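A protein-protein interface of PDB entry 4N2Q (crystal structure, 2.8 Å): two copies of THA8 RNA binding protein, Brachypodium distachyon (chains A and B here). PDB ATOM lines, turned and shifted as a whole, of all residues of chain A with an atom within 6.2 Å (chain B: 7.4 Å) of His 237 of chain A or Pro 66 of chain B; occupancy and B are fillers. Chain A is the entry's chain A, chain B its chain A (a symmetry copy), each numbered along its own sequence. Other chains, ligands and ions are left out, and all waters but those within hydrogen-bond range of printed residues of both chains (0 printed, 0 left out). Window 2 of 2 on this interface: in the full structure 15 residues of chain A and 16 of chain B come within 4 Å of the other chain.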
ATOM      1  N   ASP A 232      37.725   6.809  24.536  1.00  0.00           N
ATOM      2  CA  ASP A 232      37.243   6.441  25.844  1.00  0.00           C
ATOM      3  C   ASP A 232      36.277   7.510  26.352  1.00  0.00           C
ATOM      4  O   ASP A 232      35.202   7.198  26.903  1.00  0.00           O
ATOM      5  CB  ASP A 232      38.433   6.287  26.793  1.00  0.00           C
ATOM      6  CG  ASP A 232      38.129   5.382  27.945  1.00  0.00           C
ATOM      7  OD1 ASP A 232      37.249   5.713  28.788  1.00  0.00           O
ATOM      8  OD2 ASP A 232      38.787   4.328  28.003  1.00  0.00           O
ATOM      9  N   TRP A 233      36.673   8.772  26.159  1.00  0.00           N
ATOM     10  CA  TRP A 233      35.865   9.916  26.587  1.00  0.00           C
ATOM     11  C   TRP A 233      34.508   9.864  25.929  1.00  0.00           C
ATOM     12  O   TRP A 233      33.467   9.919  26.604  1.00  0.00           O
ATOM     13  CB  TRP A 233      36.576  11.221  26.225  1.00  0.00           C
ATOM     14  CG  TRP A 233      35.953  12.441  26.821  1.00  0.00           C
ATOM     15  CD1 TRP A 233      36.327  13.082  27.976  1.00  0.00           C
ATOM     16  CD2 TRP A 233      34.832  13.175  26.303  1.00  0.00           C
ATOM     17  NE1 TRP A 233      35.499  14.154  28.208  1.00  0.00           N
ATOM     18  CE2 TRP A 233      34.584  14.242  27.190  1.00  0.00           C
ATOM     19  CE3 TRP A 233      34.015  13.037  25.176  1.00  0.00           C
ATOM     20  CZ2 TRP A 233      33.556  15.166  26.975  1.00  0.00           C
ATOM     21  CZ3 TRP A 233      32.998  13.966  24.969  1.00  0.00           C
ATOM     22  CH2 TRP A 233      32.779  15.005  25.862  1.00  0.00           C
ATOM     23  N   GLU A 234      34.532   9.720  24.606  1.00  0.00           N
ATOM     24  CA  GLU A 234      33.311   9.621  23.813  1.00  0.00           C
ATOM     25  C   GLU A 234      32.434   8.469  24.279  1.00  0.00           C
ATOM     26  O   GLU A 234      31.217   8.580  24.348  1.00  0.00           O
ATOM     27  CB  GLU A 234      33.653   9.457  22.323  1.00  0.00           C
ATOM     28  CG  GLU A 234      34.303  10.674  21.676  1.00  0.00           C
ATOM     29  CD  GLU A 234      33.385  11.896  21.589  1.00  0.00           C
ATOM     30  OE1 GLU A 234      32.234  11.834  22.070  1.00  0.00           O
ATOM     31  OE2 GLU A 234      33.810  12.925  21.019  1.00  0.00           O
ATOM     32  N   ALA A 235      33.079   7.362  24.630  1.00  0.00           N
ATOM     33  CA  ALA A 235      32.373   6.170  25.068  1.00  0.00           C
ATOM     34  C   ALA A 235      31.600   6.405  26.361  1.00  0.00           C
ATOM     35  O   ALA A 235      30.729   5.618  26.707  1.00  0.00           O
ATOM     36  CB  ALA A 235      33.350   5.022  25.236  1.00  0.00           C
ATOM     37  N   ARG A 236      31.879   7.505  27.053  1.00  0.00           N
ATOM     38  CA  ARG A 236      31.185   7.793  28.307  1.00  0.00           C
ATOM     39  C   ARG A 236      30.273   9.003  28.260  1.00  0.00           C
ATOM     40  O   ARG A 236      29.432   9.183  29.156  1.00  0.00           O
ATOM     41  CB  ARG A 236      32.194   7.987  29.408  1.00  0.00           C
ATOM     42  CG  ARG A 236      33.143   6.806  29.586  1.00  0.00           C
ATOM     43  CD  ARG A 236      34.244   7.114  30.600  1.00  0.00           C
ATOM     44  NE  ARG A 236      34.874   8.420  30.341  1.00  0.00           N
ATOM     45  CZ  ARG A 236      36.173   8.680  30.470  1.00  0.00           C
ATOM     46  NH1 ARG A 236      36.636   9.898  30.201  1.00  0.00           N
ATOM     47  NH2 ARG A 236      37.018   7.736  30.856  1.00  0.00           N
ATOM     48  N   HIS A 237      30.415   9.836  27.234  1.00  0.00           N
ATOM     49  CA  HIS A 237      29.550  11.026  27.128  1.00  0.00           C
ATOM     50  C   HIS A 237      28.554  10.950  25.992  1.00  0.00           C
ATOM     51  O   HIS A 237      27.500  11.608  26.013  1.00  0.00           O
ATOM     52  CB  HIS A 237      30.410  12.302  27.011  1.00  0.00           C
ATOM     53  CG  HIS A 237      31.322  12.510  28.180  1.00  0.00           C
ATOM     54  ND1 HIS A 237      32.515  11.836  28.310  1.00  0.00           N
ATOM     55  CD2 HIS A 237      31.201  13.273  29.292  1.00  0.00           C
ATOM     56  CE1 HIS A 237      33.099  12.187  29.441  1.00  0.00           C
ATOM     57  NE2 HIS A 237      32.319  13.055  30.058  1.00  0.00           N
ATOM     58  N   LEU A 238      28.884  10.150  24.995  1.00  0.00           N
ATOM     59  CA  LEU A 238      28.046  10.083  23.832  1.00  0.00           C
ATOM     60  C   LEU A 238      26.799   9.373  24.347  1.00  0.00           C
ATOM     61  O   LEU A 238      26.938   8.444  25.131  1.00  0.00           O
ATOM     62  CB  LEU A 238      28.782   9.378  22.686  1.00  0.00           C
ATOM     63  CG  LEU A 238      28.830  10.115  21.328  1.00  0.00           C
ATOM     64  CD1 LEU A 238      29.008  11.635  21.408  1.00  0.00           C
ATOM     65  CD2 LEU A 238      29.931   9.484  20.479  1.00  0.00           C
ATOM     66  N   PRO A 239      25.594   9.916  24.063  1.00  0.00           N
ATOM     67  CA  PRO A 239      24.347   9.215  24.328  1.00  0.00           C
ATOM     68  C   PRO A 239      24.419   7.888  23.604  1.00  0.00           C
ATOM     69  O   PRO A 239      24.571   7.865  22.383  1.00  0.00           O
ATOM     70  CB  PRO A 239      23.267  10.153  23.742  1.00  0.00           C
ATOM     71  CG  PRO A 239      23.994  11.323  23.158  1.00  0.00           C
ATOM     72  CD  PRO A 239      25.346  11.340  23.808  1.00  0.00           C
ATOM     73  N   ASP A 240      24.373   6.812  24.388  1.00  0.00           N
ATOM     74  CA  ASP A 240      24.613   5.392  23.968  1.00  0.00           C
ATOM     75  C   ASP A 240      23.618   4.687  23.006  1.00  0.00           C
ATOM     76  O   ASP A 240      24.026   4.086  22.010  1.00  0.00           O
ATOM     77  CB  ASP A 240      24.688   4.527  25.231  1.00  0.00           C
ATOM     78  CG  ASP A 240      23.493   4.736  26.144  1.00  0.00           C
ATOM     79  OD1 ASP A 240      23.272   5.907  26.554  1.00  0.00           O
ATOM     80  OD2 ASP A 240      22.771   3.742  26.413  1.00  0.00           O
ATOM     81  N   THR B  60      28.109  23.356  30.453  1.00  0.00           N
ATOM     82  CA  THR B  60      28.511  21.940  30.443  1.00  0.00           C
ATOM     83  C   THR B  60      29.909  21.728  31.021  1.00  0.00           C
ATOM     84  O   THR B  60      30.299  20.600  31.271  1.00  0.00           O
ATOM     85  CB  THR B  60      28.491  21.371  29.017  1.00  0.00           C
ATOM     86  OG1 THR B  60      29.218  22.258  28.150  1.00  0.00           O
ATOM     87  CG2 THR B  60      27.038  21.207  28.526  1.00  0.00           C
ATOM     88  N   ASP B  63      29.714  20.636  34.515  1.00  0.00           N
ATOM     89  CA  ASP B  63      29.146  19.286  34.559  1.00  0.00           C
ATOM     90  C   ASP B  63      29.215  18.652  33.173  1.00  0.00           C
ATOM     91  O   ASP B  63      28.381  18.932  32.302  1.00  0.00           O
ATOM     92  CB  ASP B  63      27.698  19.337  35.073  1.00  0.00           C
ATOM     93  CG  ASP B  63      27.146  17.953  35.463  1.00  0.00           C
ATOM     94  OD1 ASP B  63      27.502  16.929  34.830  1.00  0.00           O
ATOM     95  OD2 ASP B  63      26.325  17.890  36.404  1.00  0.00           O
ATOM     96  N   ARG B  64      30.211  17.795  32.981  1.00  0.00           N
ATOM     97  CA  ARG B  64      30.432  17.138  31.685  1.00  0.00           C
ATOM     98  C   ARG B  64      29.386  16.066  31.371  1.00  0.00           C
ATOM     99  O   ARG B  64      29.234  15.679  30.209  1.00  0.00           O
ATOM    100  CB  ARG B  64      31.822  16.500  31.639  1.00  0.00           C
ATOM    101  CG  ARG B  64      32.964  17.414  32.044  1.00  0.00           C
ATOM    102  CD  ARG B  64      33.362  18.387  30.938  1.00  0.00           C
ATOM    103  NE  ARG B  64      34.589  19.086  31.332  1.00  0.00           N
ATOM    104  CZ  ARG B  64      35.170  20.078  30.665  1.00  0.00           C
ATOM    105  NH1 ARG B  64      34.661  20.533  29.524  1.00  0.00           N
ATOM    106  NH2 ARG B  64      36.272  20.625  31.151  1.00  0.00           N
ATOM    107  N   SER B  65      28.673  15.591  32.399  1.00  0.00           N
ATOM    108  CA  SER B  65      27.722  14.497  32.243  1.00  0.00           C
ATOM    109  C   SER B  65      26.717  14.809  31.136  1.00  0.00           C
ATOM    110  O   SER B  65      26.238  15.941  31.052  1.00  0.00           O
ATOM    111  CB  SER B  65      26.986  14.215  33.559  1.00  0.00           C
ATOM    112  OG  SER B  65      25.898  15.097  33.753  1.00  0.00           O
ATOM    113  N   PRO B  66      26.407  13.815  30.280  1.00  0.00           N
ATOM    114  CA  PRO B  66      25.430  13.999  29.187  1.00  0.00           C
ATOM    115  C   PRO B  66      24.006  14.365  29.621  1.00  0.00           C
ATOM    116  O   PRO B  66      23.316  15.066  28.873  1.00  0.00           O
ATOM    117  CB  PRO B  66      25.421  12.638  28.460  1.00  0.00           C
ATOM    118  CG  PRO B  66      26.038  11.691  29.407  1.00  0.00           C
ATOM    119  CD  PRO B  66      27.019  12.478  30.233  1.00  0.00           C
ATOM    120  N   PRO B  67      23.549  13.896  30.803  1.00  0.00           N
ATOM    121  CA  PRO B  67      22.186  14.288  31.183  1.00  0.00           C
ATOM    122  C   PRO B  67      22.040  15.802  31.376  1.00  0.00           C
ATOM    123  O   PRO B  67      21.076  16.399  30.896  1.00  0.00           O
ATOM    124  CB  PRO B  67      21.966  13.532  32.494  1.00  0.00           C
ATOM    125  CG  PRO B  67      22.904  12.366  32.419  1.00  0.00           C
ATOM    126  CD  PRO B  67      24.118  12.931  31.761  1.00  0.00           C
ATOM    127  N   ALA B  68      23.006  16.412  32.053  1.00  0.00           N
ATOM    128  CA  ALA B  68      23.012  17.865  32.259  1.00  0.00           C
ATOM    129  C   ALA B  68      23.411  18.589  30.985  1.00  0.00           C
ATOM    130  O   ALA B  68      23.026  19.732  30.758  1.00  0.00           O
ATOM    131  CB  ALA B  68      23.965  18.248  33.383  1.00  0.00           C
ATOM    132  N   ALA B  69      24.189  17.914  30.151  1.00  0.00           N
ATOM    133  CA  ALA B  69      24.635  18.487  28.882  1.00  0.00           C
ATOM    134  C   ALA B  69      23.449  18.763  27.957  1.00  0.00           C
ATOM    135  O   ALA B  69      23.428  19.754  27.226  1.00  0.00           O
ATOM    136  CB  ALA B  69      25.633  17.558  28.205  1.00  0.00           C
ATOM    137  N   THR B  70      22.465  17.878  28.008  1.00  0.00           N
ATOM    138  CA  THR B  70      21.242  18.046  27.244  1.00  0.00           C
ATOM    139  C   THR B  70      20.447  19.245  27.742  1.00  0.00           C
ATOM    140  O   THR B  70      19.994  20.084  26.956  1.00  0.00           O
ATOM    141  CB  THR B  70      20.347  16.796  27.348  1.00  0.00           C
ATOM    142  OG1 THR B  70      21.106  15.647  26.953  1.00  0.00           O
ATOM    143  CG2 THR B  70      19.113  16.923  26.443  1.00  0.00           C
ATOM    144  N   ALA B  71      20.272  19.310  29.060  1.00  0.00           N
ATOM    145  CA  ALA B  71      19.517  20.391  29.677  1.00  0.00           C
ATOM    146  C   ALA B  71      20.208  21.730  29.439  1.00  0.00           C
ATOM    147  O   ALA B  71      19.555  22.767  29.398  1.00  0.00           O
ATOM    148  CB  ALA B  71      19.335  20.133  31.161  1.00  0.00           C
ATOM    149  N   ALA B  72      21.523  21.704  29.260  1.00  0.00           N
ATOM    150  CA  ALA B  72      22.271  22.931  28.999  1.00  0.00           C
ATOM    151  C   ALA B  72      22.068  23.382  27.569  1.00  0.00           C
ATOM    152  O   ALA B  72      22.085  24.591  27.292  1.00  0.00           O
ATOM    153  CB  ALA B  72      23.751  22.720  29.271  1.00  0.00           C
ATOM    154  N   SER B  99      30.038  15.935  20.598  1.00  0.00           N
ATOM    155  CA  SER B  99      28.943  15.558  21.497  1.00  0.00           C
ATOM    156  C   SER B  99      27.996  16.717  21.732  1.00  0.00           C
ATOM    157  O   SER B  99      26.804  16.521  21.907  1.00  0.00           O
ATOM    158  CB  SER B  99      29.461  15.040  22.856  1.00  0.00           C
ATOM    159  OG  SER B  99      29.917  16.090  23.699  1.00  0.00           O
ATOM    160  N   ALA B 103      24.097  17.338  20.682  1.00  0.00           N
ATOM    161  CA  ALA B 103      23.106  17.850  21.624  1.00  0.00           C
ATOM    162  C   ALA B 103      22.276  18.938  20.941  1.00  0.00           C
ATOM    163  O   ALA B 103      21.052  19.004  21.094  1.00  0.00           O
ATOM    164  CB  ALA B 103      23.801  18.404  22.847  1.00  0.00           C
ATOM    165  N   ALA B 134      32.853   4.380  19.533  1.00  0.00           N
ATOM    166  CA  ALA B 134      31.623   5.052  19.965  1.00  0.00           C
ATOM    167  C   ALA B 134      31.102   5.990  18.885  1.00  0.00           C
ATOM    168  O   ALA B 134      29.918   5.946  18.514  1.00  0.00           O
ATOM    169  CB  ALA B 134      31.862   5.813  21.265  1.00  0.00           C
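Printed residues of chain B that touch a printed residue of chain A: Arg 64, Pro 66, Ser 99 and Ala 134.
Among the printed residues, 5 pairs touch across the chains.
Among the printed residues, no Asp or Glu carboxylate lies within 4 Å of a Lys or Arg side-chain nitrogen of the other chain.
Printed residues of chain B within 4 Å of His 237 of chain A: Arg 64 (3.2 Å) and Pro 66 (3.4 Å).
Of the printed residues of chain B, Leu 238 of chain A touches Ser 99 (3.7 Å).
Printed residues of chain A within 4 Å of Arg 64 of chain B: His 237 (3.2 Å).
Of chain A, only His 237 comes within 4 Å of Pro 66 of chain B.
Of the printed residues of chain A, Ser 99 of chain B touches Trp 233 (3.7 Å) and Leu 238 (3.7 Å).
Printed residues of chain A within 4 Å of Ala 134 of chain B: Ala 235.
The nearest residue of chain B that does not touch His 237 of chain A is Ser 65 of chain B (4.6 Å).
The backbone carbonyl oxygen of Trp 233 of chain A sits at hydrogen-bond distance from a ring nitrogen (ND1) of His 237 of chain A, at 2.7 Å.
O of Pro 66 of chain B lies within hydrogen-bond range of OG1 of Thr 70 of chain B (3.0 Å).
No position is printed for both chains.
Among the printed residues, merely in contact across the chains: Trp 233 of chain A with Ser 99 of chain B (3.7 Å), Ala 235 of chain A with Ala 134 of chain B (3.9 Å), His 237 of chain A with Arg 64 of chain B (3.2 Å), His 237 of chain A with Pro 66 of chain B (3.4 Å) and Leu 238 of chain A with Ser 99 of chain B (3.7 Å).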
